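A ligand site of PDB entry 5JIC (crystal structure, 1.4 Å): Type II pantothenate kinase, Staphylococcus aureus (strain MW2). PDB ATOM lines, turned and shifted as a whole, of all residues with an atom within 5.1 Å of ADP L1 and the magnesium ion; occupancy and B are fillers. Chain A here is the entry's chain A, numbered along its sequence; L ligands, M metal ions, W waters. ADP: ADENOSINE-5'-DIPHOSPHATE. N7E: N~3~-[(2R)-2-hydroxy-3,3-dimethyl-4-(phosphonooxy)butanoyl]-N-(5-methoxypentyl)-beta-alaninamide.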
ATOM      1  N   ASP A   6       5.169   6.535  23.784  1.00  0.00           N
ATOM      2  CA  ASP A   6       5.086   5.440  24.744  1.00  0.00           C
ATOM      3  C   ASP A   6       5.049   4.166  23.897  1.00  0.00           C
ATOM      4  O   ASP A   6       4.014   3.833  23.273  1.00  0.00           O
ATOM      5  CB  ASP A   6       3.830   5.605  25.623  1.00  0.00           C
ATOM      6  CG  ASP A   6       3.610   4.461  26.576  1.00  0.00           C
ATOM      7  OD1 ASP A   6       4.404   3.512  26.582  1.00  0.00           O
ATOM      8  OD2 ASP A   6       2.665   4.572  27.354  1.00  0.00           O
ATOM      9  N   GLY A   8       4.913   0.663  23.836  1.00  0.00           N
ATOM     10  CA  GLY A   8       4.531  -0.411  24.748  1.00  0.00           C
ATOM     11  C   GLY A   8       4.691  -1.794  24.129  1.00  0.00           C
ATOM     12  O   GLY A   8       5.293  -1.941  23.047  1.00  0.00           O
ATOM     13  N   GLY A   9       4.142  -2.792  24.805  1.00  0.00           N
ATOM     14  CA  GLY A   9       4.267  -4.181  24.339  1.00  0.00           C
ATOM     15  C   GLY A   9       3.489  -4.486  23.070  1.00  0.00           C
ATOM     16  O   GLY A   9       3.858  -5.385  22.325  1.00  0.00           O
ATOM     17  N   THR A  10       2.412  -3.734  22.829  1.00  0.00           N
ATOM     18  CA  THR A  10       1.549  -3.990  21.649  1.00  0.00           C
ATOM     19  C   THR A  10       1.350  -2.772  20.777  1.00  0.00           C
ATOM     20  O   THR A  10       1.325  -2.901  19.548  1.00  0.00           O
ATOM     21  CB  THR A  10       0.200  -4.577  22.088  1.00  0.00           C
ATOM     22  OG1 THR A  10       0.442  -5.774  22.797  1.00  0.00           O
ATOM     23  CG2 THR A  10      -0.706  -4.920  20.888  1.00  0.00           C
ATOM     24  N   LEU A  11       1.179  -1.613  21.385  1.00  0.00           N
ATOM     25  CA  LEU A  11       0.977  -0.372  20.654  1.00  0.00           C
ATOM     26  C   LEU A  11       2.001   0.685  21.023  1.00  0.00           C
ATOM     27  O   LEU A  11       2.434   0.797  22.172  1.00  0.00           O
ATOM     28  CB  LEU A  11      -0.419   0.208  20.873  1.00  0.00           C
ATOM     29  CG  LEU A  11      -1.610  -0.695  20.506  1.00  0.00           C
ATOM     30  CD1 LEU A  11      -2.910  -0.053  20.909  1.00  0.00           C
ATOM     31  CD2 LEU A  11      -1.629  -1.002  19.030  1.00  0.00           C
ATOM     32  N   LYS A  13       2.169   4.599  21.188  1.00  0.00           N
ATOM     33  CA  LYS A  13       1.296   5.758  21.301  1.00  0.00           C
ATOM     34  C   LYS A  13       2.153   6.987  21.109  1.00  0.00           C
ATOM     35  O   LYS A  13       3.157   7.141  21.792  1.00  0.00           O
ATOM     36  CB  LYS A  13       0.637   5.846  22.669  1.00  0.00           C
ATOM     37  CG  LYS A  13      -0.554   4.896  22.881  1.00  0.00           C
ATOM     38  CD  LYS A  13      -0.210   3.386  22.970  1.00  0.00           C
ATOM     39  CE  LYS A  13       0.700   3.073  24.168  1.00  0.00           C
ATOM     40  NZ  LYS A  13       0.851   1.609  24.331  1.00  0.00           N
ATOM     41  N   LEU A  28       1.280  -0.144  15.532  1.00  0.00           N
ATOM     42  CA  LEU A  28       1.588  -1.431  16.192  1.00  0.00           C
ATOM     43  C   LEU A  28       3.076  -1.484  16.555  1.00  0.00           C
ATOM     44  O   LEU A  28       3.949  -1.118  15.761  1.00  0.00           O
ATOM     45  CB  LEU A  28       1.249  -2.615  15.265  1.00  0.00           C
ATOM     46  CG  LEU A  28      -0.217  -2.704  14.880  1.00  0.00           C
ATOM     47  CD1 LEU A  28      -0.378  -3.900  13.956  1.00  0.00           C
ATOM     48  CD2 LEU A  28      -1.141  -2.836  16.084  1.00  0.00           C
ATOM     49  N   THR A  29       3.365  -1.959  17.742  1.00  0.00           N
ATOM     50  CA  THR A  29       4.736  -2.193  18.144  1.00  0.00           C
ATOM     51  C   THR A  29       5.484  -3.087  17.130  1.00  0.00           C
ATOM     52  O   THR A  29       6.674  -2.874  16.872  1.00  0.00           O
ATOM     53  CB  THR A  29       4.769  -2.780  19.564  1.00  0.00           C
ATOM     54  OG1 THR A  29       4.156  -1.822  20.420  1.00  0.00           O
ATOM     55  CG2 THR A  29       6.203  -3.038  20.007  1.00  0.00           C
ATOM     56  N   GLU A  70       7.867   4.280  32.714  1.00  0.00           N
ATOM     57  CA  GLU A  70       6.474   4.350  32.324  1.00  0.00           C
ATOM     58  C   GLU A  70       5.559   4.641  33.450  1.00  0.00           C
ATOM     59  O   GLU A  70       4.548   5.263  33.232  1.00  0.00           O
ATOM     60  CB  GLU A  70       6.000   3.116  31.499  1.00  0.00           C
ATOM     61  CG  GLU A  70       5.930   1.784  32.225  1.00  0.00           C
ATOM     62  CD  GLU A  70       5.355   0.673  31.363  1.00  0.00           C
ATOM     63  OE1 GLU A  70       4.139   0.588  31.233  1.00  0.00           O
ATOM     64  OE2 GLU A  70       6.132  -0.104  30.808  1.00  0.00           O
ATOM     65  N   ASN A  96      -3.752   0.315  34.782  1.00  0.00           N
ATOM     66  CA  ASN A  96      -3.263   0.462  33.436  1.00  0.00           C
ATOM     67  C   ASN A  96      -3.398  -0.896  32.742  1.00  0.00           C
ATOM     68  O   ASN A  96      -2.550  -1.784  32.904  1.00  0.00           O
ATOM     69  CB  ASN A  96      -1.823   0.964  33.467  1.00  0.00           C
ATOM     70  CG  ASN A  96      -1.319   1.372  32.133  1.00  0.00           C
ATOM     71  OD1 ASN A  96      -1.955   1.152  31.109  1.00  0.00           O
ATOM     72  ND2 ASN A  96      -0.145   1.992  32.145  1.00  0.00           N
ATOM     73  N   VAL A  97      -4.459  -1.023  31.968  1.00  0.00           N
ATOM     74  CA  VAL A  97      -4.830  -2.305  31.361  1.00  0.00           C
ATOM     75  C   VAL A  97      -4.278  -2.289  29.944  1.00  0.00           C
ATOM     76  O   VAL A  97      -4.974  -1.934  28.960  1.00  0.00           O
ATOM     77  CB  VAL A  97      -6.345  -2.520  31.375  1.00  0.00           C
ATOM     78  CG1 VAL A  97      -6.662  -3.938  30.904  1.00  0.00           C
ATOM     79  CG2 VAL A  97      -6.891  -2.274  32.779  1.00  0.00           C
ATOM     80  N   GLY A  98      -3.000  -2.618  29.860  1.00  0.00           N
ATOM     81  CA  GLY A  98      -2.267  -2.632  28.588  1.00  0.00           C
ATOM     82  C   GLY A  98      -2.134  -4.035  28.071  1.00  0.00           C
ATOM     83  O   GLY A  98      -3.041  -4.850  28.210  1.00  0.00           O
ATOM     84  N   THR A  99      -0.980  -4.367  27.518  1.00  0.00           N
ATOM     85  CA  THR A  99      -0.740  -5.721  27.119  1.00  0.00           C
ATOM     86  C   THR A  99      -0.909  -6.617  28.361  1.00  0.00           C
ATOM     87  O   THR A  99      -1.513  -7.694  28.283  1.00  0.00           O
ATOM     88  CB  THR A  99       0.644  -5.911  26.522  1.00  0.00           C
ATOM     89  OG1 THR A  99       0.789  -5.058  25.370  1.00  0.00           O
ATOM     90  CG2 THR A  99       0.863  -7.352  26.098  1.00  0.00           C
ATOM     91  N   GLY A 100      -0.356  -6.173  29.483  1.00  0.00           N
ATOM     92  CA  GLY A 100      -0.681  -6.706  30.808  1.00  0.00           C
ATOM     93  C   GLY A 100      -1.160  -5.563  31.680  1.00  0.00           C
ATOM     94  O   GLY A 100      -1.206  -4.419  31.224  1.00  0.00           O
ATOM     95  N   GLY A 121      -4.994  -6.845  27.920  1.00  0.00           N
ATOM     96  CA  GLY A 121      -5.256  -6.851  26.496  1.00  0.00           C
ATOM     97  C   GLY A 121      -4.556  -7.931  25.704  1.00  0.00           C
ATOM     98  O   GLY A 121      -5.085  -8.431  24.685  1.00  0.00           O
ATOM     99  N   GLY A 122      -3.365  -8.295  26.123  1.00  0.00           N
ATOM    100  CA  GLY A 122      -2.634  -9.402  25.498  1.00  0.00           C
ATOM    101  C   GLY A 122      -3.337 -10.723  25.602  1.00  0.00           C
ATOM    102  O   GLY A 122      -3.369 -11.510  24.636  1.00  0.00           O
ATOM    103  N   ILE A 124      -6.625 -11.041  26.033  1.00  0.00           N
ATOM    104  CA  ILE A 124      -7.796 -10.919  25.155  1.00  0.00           C
ATOM    105  C   ILE A 124      -7.422 -11.337  23.733  1.00  0.00           C
ATOM    106  O   ILE A 124      -8.080 -12.169  23.101  1.00  0.00           O
ATOM    107  CB  ILE A 124      -8.404  -9.505  25.206  1.00  0.00           C
ATOM    108  CG1 ILE A 124      -9.033  -9.280  26.601  1.00  0.00           C
ATOM    109  CG2 ILE A 124      -9.444  -9.310  24.128  1.00  0.00           C
ATOM    110  CD1 ILE A 124      -9.502  -7.872  26.896  1.00  0.00           C
ATOM    111  N   GLN A 125      -6.344 -10.771  23.220  1.00  0.00           N
ATOM    112  CA  GLN A 125      -5.927 -11.120  21.867  1.00  0.00           C
ATOM    113  C   GLN A 125      -5.453 -12.565  21.726  1.00  0.00           C
ATOM    114  O   GLN A 125      -5.815 -13.230  20.761  1.00  0.00           O
ATOM    115  CB  GLN A 125      -4.793 -10.202  21.409  1.00  0.00           C
ATOM    116  CG  GLN A 125      -5.238  -8.758  21.199  1.00  0.00           C
ATOM    117  CD  GLN A 125      -4.186  -7.949  20.572  1.00  0.00           C
ATOM    118  OE1 GLN A 125      -4.154  -7.770  19.317  1.00  0.00           O
ATOM    119  NE2 GLN A 125      -3.281  -7.470  21.375  1.00  0.00           N
ATOM    120  N   TYR A 137      -7.774  -7.240  15.472  1.00  0.00           N
ATOM    121  CA  TYR A 137      -8.256  -6.743  16.754  1.00  0.00           C
ATOM    122  C   TYR A 137      -9.699  -6.211  16.653  1.00  0.00           C
ATOM    123  O   TYR A 137     -10.523  -6.493  17.505  1.00  0.00           O
ATOM    124  CB  TYR A 137      -7.332  -5.631  17.284  1.00  0.00           C
ATOM    125  CG  TYR A 137      -7.830  -5.058  18.592  1.00  0.00           C
ATOM    126  CD1 TYR A 137      -7.660  -5.754  19.795  1.00  0.00           C
ATOM    127  CD2 TYR A 137      -8.566  -3.873  18.606  1.00  0.00           C
ATOM    128  CE1 TYR A 137      -8.144  -5.255  20.969  1.00  0.00           C
ATOM    129  CE2 TYR A 137      -9.064  -3.354  19.781  1.00  0.00           C
ATOM    130  CZ  TYR A 137      -8.864  -4.059  20.973  1.00  0.00           C
ATOM    131  OH  TYR A 137      -9.308  -3.564  22.167  1.00  0.00           O
ATOM    132  N   GLY A 224      -5.563   2.478  29.555  1.00  0.00           N
ATOM    133  CA  GLY A 224      -5.022   1.442  28.689  1.00  0.00           C
ATOM    134  C   GLY A 224      -5.785   1.304  27.371  1.00  0.00           C
ATOM    135  O   GLY A 224      -7.027   1.550  27.287  1.00  0.00           O
ATOM    136  N   SER A 225      -5.105   0.820  26.359  1.00  0.00           N
ATOM    137  CA  SER A 225      -5.743   0.673  25.051  1.00  0.00           C
ATOM    138  C   SER A 225      -6.706  -0.519  25.009  1.00  0.00           C
ATOM    139  O   SER A 225      -7.461  -0.668  24.067  1.00  0.00           O
ATOM    140  CB  SER A 225      -4.716   0.561  23.937  1.00  0.00           C
ATOM    141  OG  SER A 225      -3.803   1.642  23.938  1.00  0.00           O
ATOM    142  N   SER A 226      -6.683  -1.382  26.032  1.00  0.00           N
ATOM    143  CA  SER A 226      -7.539  -2.560  26.059  1.00  0.00           C
ATOM    144  C   SER A 226      -9.038  -2.245  26.021  1.00  0.00           C
ATOM    145  O   SER A 226      -9.849  -3.087  25.648  1.00  0.00           O
ATOM    146  CB  SER A 226      -7.221  -3.370  27.286  1.00  0.00           C
ATOM    147  OG  SER A 226      -5.908  -3.868  27.280  1.00  0.00           O
ATOM    148  N   HIS A 228     -10.268   0.148  24.117  1.00  0.00           N
ATOM    149  CA  HIS A 228     -10.612   0.678  22.808  1.00  0.00           C
ATOM    150  C   HIS A 228     -11.395  -0.327  21.984  1.00  0.00           C
ATOM    151  O   HIS A 228     -11.005  -1.483  21.866  1.00  0.00           O
ATOM    152  CB  HIS A 228      -9.370   1.053  22.020  1.00  0.00           C
ATOM    153  CG  HIS A 228      -9.664   1.407  20.587  1.00  0.00           C
ATOM    154  ND1 HIS A 228     -10.274   2.590  20.235  1.00  0.00           N
ATOM    155  CD2 HIS A 228      -9.471   0.717  19.439  1.00  0.00           C
ATOM    156  CE1 HIS A 228     -10.435   2.621  18.926  1.00  0.00           C
ATOM    157  NE2 HIS A 228      -9.964   1.506  18.421  1.00  0.00           N
HETATM  158  PB  ADP L   1       0.952  -1.488  25.672  1.00  0.00           P
HETATM  159  O1B ADP L   1       1.467  -2.771  26.319  1.00  0.00           O
HETATM  160  O2B ADP L   1       1.422  -0.261  26.394  1.00  0.00           O
HETATM  161  O3B ADP L   1       1.175  -1.475  24.192  1.00  0.00           O
HETATM  162  PA  ADP L   1      -1.856  -0.653  25.566  1.00  0.00           P
HETATM  163  O1A ADP L   1      -1.547   0.103  24.306  1.00  0.00           O
HETATM  164  O2A ADP L   1      -2.306   0.127  26.735  1.00  0.00           O
HETATM  165  O3A ADP L   1      -0.619  -1.554  25.899  1.00  0.00           O
HETATM  166  O5' ADP L   1      -2.947  -1.777  25.299  1.00  0.00           O
HETATM  167  C5' ADP L   1      -2.701  -2.790  24.336  1.00  0.00           C
HETATM  168  C4' ADP L   1      -3.970  -3.577  24.158  1.00  0.00           C
HETATM  169  O4' ADP L   1      -4.991  -2.742  23.628  1.00  0.00           O
HETATM  170  C3' ADP L   1      -3.874  -4.731  23.177  1.00  0.00           C
HETATM  171  O3' ADP L   1      -3.348  -5.900  23.845  1.00  0.00           O
HETATM  172  C2' ADP L   1      -5.311  -4.878  22.693  1.00  0.00           C
HETATM  173  O2' ADP L   1      -6.096  -5.654  23.626  1.00  0.00           O
HETATM  174  C1' ADP L   1      -5.821  -3.466  22.729  1.00  0.00           C
HETATM  175  N9  ADP L   1      -5.826  -2.787  21.401  1.00  0.00           N
HETATM  176  C8  ADP L   1      -6.526  -1.655  21.252  1.00  0.00           C
HETATM  177  N7  ADP L   1      -6.439  -1.224  19.983  1.00  0.00           N
HETATM  178  C5  ADP L   1      -5.661  -2.078  19.322  1.00  0.00           C
HETATM  179  C6  ADP L   1      -5.178  -2.202  17.958  1.00  0.00           C
HETATM  180  N6  ADP L   1      -5.531  -1.275  17.057  1.00  0.00           N
HETATM  181  N1  ADP L   1      -4.401  -3.259  17.653  1.00  0.00           N
HETATM  182  C2  ADP L   1      -4.043  -4.194  18.583  1.00  0.00           C
HETATM  183  N3  ADP L   1      -4.442  -4.125  19.848  1.00  0.00           N
HETATM  184  C4  ADP L   1      -5.245  -3.115  20.235  1.00  0.00           C
HETATM  185  O01 N7E L   2       1.482  -3.606  29.549  1.00  0.00           O
HETATM  186  P02 N7E L   2       2.576  -2.476  29.274  1.00  0.00           P
HETATM  187  O03 N7E L   2       1.994  -1.047  29.215  1.00  0.00           O
HETATM  188  O04 N7E L   2       3.377  -2.757  28.018  1.00  0.00           O
HETATM  189  O05 N7E L   2       3.604  -2.500  30.531  1.00  0.00           O
HETATM  190  C06 N7E L   2       4.472  -3.561  30.812  1.00  0.00           C
HETATM  191  C07 N7E L   2       4.198  -4.142  32.194  1.00  0.00           C
HETATM  192  C08 N7E L   2       4.581  -3.042  33.251  1.00  0.00           C
HETATM  193  C09 N7E L   2       5.155  -5.309  32.325  1.00  0.00           C
HETATM  194  C10 N7E L   2       2.718  -4.571  32.351  1.00  0.00           C
HETATM  195  O11 N7E L   2       2.321  -5.415  31.242  1.00  0.00           O
HETATM  196  C12 N7E L   2       2.493  -5.319  33.676  1.00  0.00           C
HETATM  197  O13 N7E L   2       2.622  -4.752  34.778  1.00  0.00           O
HETATM  198  N14 N7E L   2       2.191  -6.601  33.535  1.00  0.00           N
HETATM  199  C15 N7E L   2       1.921  -7.434  34.730  1.00  0.00           C
HETATM  200  C16 N7E L   2       3.234  -7.904  35.388  1.00  0.00           C
HETATM  201  C17 N7E L   2       2.871  -8.504  36.725  1.00  0.00           C
HETATM  202  O18 N7E L   2       2.712  -7.789  37.708  1.00  0.00           O
HETATM  203  N19 N7E L   2       2.704  -9.840  36.776  1.00  0.00           N
HETATM  204  C20 N7E L   2       2.304 -10.477  38.000  1.00  0.00           C
HETATM  205  C21 N7E L   2       2.124 -11.970  37.877  1.00  0.00           C
HETATM  206  C22 N7E L   2       3.463 -12.697  37.784  1.00  0.00           C
HETATM  207  C23 N7E L   2       3.290 -14.190  37.959  1.00  0.00           C
HETATM  208  C24 N7E L   2       4.542 -15.001  38.006  1.00  0.00           C
HETATM  209  O25 N7E L   2       5.395 -14.789  36.871  1.00  0.00           O
HETATM  210  C26 N7E L   2       6.508 -15.671  36.841  1.00  0.00           C
HETATM  211 MG    MG M   1       1.667   0.567  28.232  1.00  0.00          MG
HETATM  212  O   HOH W   1      -1.540   2.806  26.894  1.00  0.00           O
HETATM  213  O   HOH W   2      -2.356  -6.794  17.075  1.00  0.00           O
HETATM  214  O   HOH W   3       3.689   1.118  27.814  1.00  0.00           O
HETATM  215  O   HOH W   4      -0.375   0.314  28.728  1.00  0.00           O
HETATM  216  O   HOH W   5       1.156   2.377  27.393  1.00  0.00           O
HETATM  217  O   HOH W   6      -6.032   1.678  19.808  1.00  0.00           O
HETATM  218  O   HOH W   7       1.940   1.577  30.069  1.00  0.00           O
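Residues that only touch the magnesium ion: Glu 70. Of the 23 residues printed, 1 comes within 4 Å of the magnesium ion. The nearest printed residue that does not touch the magnesium ion is Lys 13 (4.1 Å).
Water W7 bridges the side-chain carboxylate (OE1) of Glu 70 (2.7 Å) and the side-chain amide nitrogen (ND2) of Asn 96 (3.0 Å). Water W3 lies within hydrogen-bond range of the side-chain carboxylate (OD1) of Asp 6 (2.8 Å) and the side-chain carboxylate (OE1) of Glu 70 (3.5 Å). Water W5 lies within hydrogen-bond range of OD2 of Asp 6 (2.7 Å) and NZ of Lys 13 (3.2 Å). Water W4 bridges an oxygen (O2A) of ADP L1 (2.8 Å) and the side-chain amide oxygen (OD1) of Asn 96 (3.0 Å).
O01 of N7E L2 sits at hydrogen-bond distance from N of Thr 99, at 3.3 Å. N of Gly 122 lies within hydrogen-bond range of O3' of ADP L1 (3.3 Å). An oxygen (O1B) of ADP L1 lies within hydrogen-bond range of the backbone NH (N) of Thr 99 (3.2 Å). N of Ser 225 sits at hydrogen-bond distance from O2A of ADP L1, 2.9 Å away. The side-chain amide nitrogen of Gln 125 is in hydrogen-bond range of an oxygen (O3') of ADP L1, 2.9 Å away. An oxygen (O01) of N7E L2 is in hydrogen-bond range of the backbone NH of Gly 100 (3.2 Å). O of Gly 121 sits at hydrogen-bond distance from O2' of ADP L1, at 3.1 Å. OG of Ser 225 is in hydrogen-bond range of O1A of ADP L1, 2.8 Å away. The backbone NH (N) of Ser 226 sits at hydrogen-bond distance from an oxygen (O4') of ADP L1 (3.2 Å). The backbone NH of Gly 9 is in hydrogen-bond range of an oxygen (O1B) of ADP L1, 3.1 Å away. The side-chain hydroxyl of Thr 99 is in hydrogen-bond range of an oxygen (O1B) of ADP L1 (2.6 Å). NZ of Lys 13 is in salt-bridge range of O1A of ADP L1, 2.8 Å away. N of Gly 9 sits at hydrogen-bond distance from O04 of N7E L2 (3.3 Å). N of Thr 10 is in hydrogen-bond range of O3B of ADP L1. N of Leu 11 lies within hydrogen-bond range of O3B of ADP L1, at 2.8 Å.
The side-chain hydroxyl of Ser 226 sits at hydrogen-bond distance from the backbone carbonyl oxygen of Gly 98, at 3.2 Å. The backbone NH of Leu 11 is in hydrogen-bond range of the side-chain hydroxyl of Thr 29, at 3.1 Å. OG1 of Thr 99 sits at hydrogen-bond distance from OG1 of Thr 10, 2.7 Å away. The side-chain hydroxyl of Tyr 137 sits at hydrogen-bond distance from the backbone carbonyl oxygen of His 228, at 2.7 Å. The side-chain hydroxyl (OG) of Ser 226 sits close to the backbone NH (N) of Gly 121 (3.2 Å). O of Gly 8 sits at hydrogen-bond distance from OG1 of Thr 29 (2.9 Å). The backbone NH (N) of Lys 13 is in hydrogen-bond range of the backbone carbonyl oxygen (O) of Asp 6 (2.9 Å). OG of Ser 226 is in hydrogen-bond range of O of Val 97 (2.7 Å).
The magnesium ion is bound by an oxygen (O03) of N7E L2 (1.9 Å), an oxygen (O2B) of ADP L1 (2.0 Å), water W5 (2.1 Å), water W7 (2.1 Å), water W4 (2.1 Å) and water W3 (2.1 Å). The magnesium ion has six donor atoms within binding distance.
Gly 8 touches ADP L1 (CA to O2B, 3.5 Å). Leu 28 touches ADP L1 (CD2 to N1, 3.6 Å). Gly 98 touches ADP L1 (CA to O2A, 3.3 Å). Tyr 137 touches ADP L1 (CZ to N9, 3.3 Å). Gly 224 touches ADP L1. His 228 touches ADP L1. Hydrophobic or aromatic side chains within 4 Å of ADP L1: Leu 11, Leu 28, Tyr 137 and His 228. Of the 23 residues printed, 16 come within 4 Å of ADP L1.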
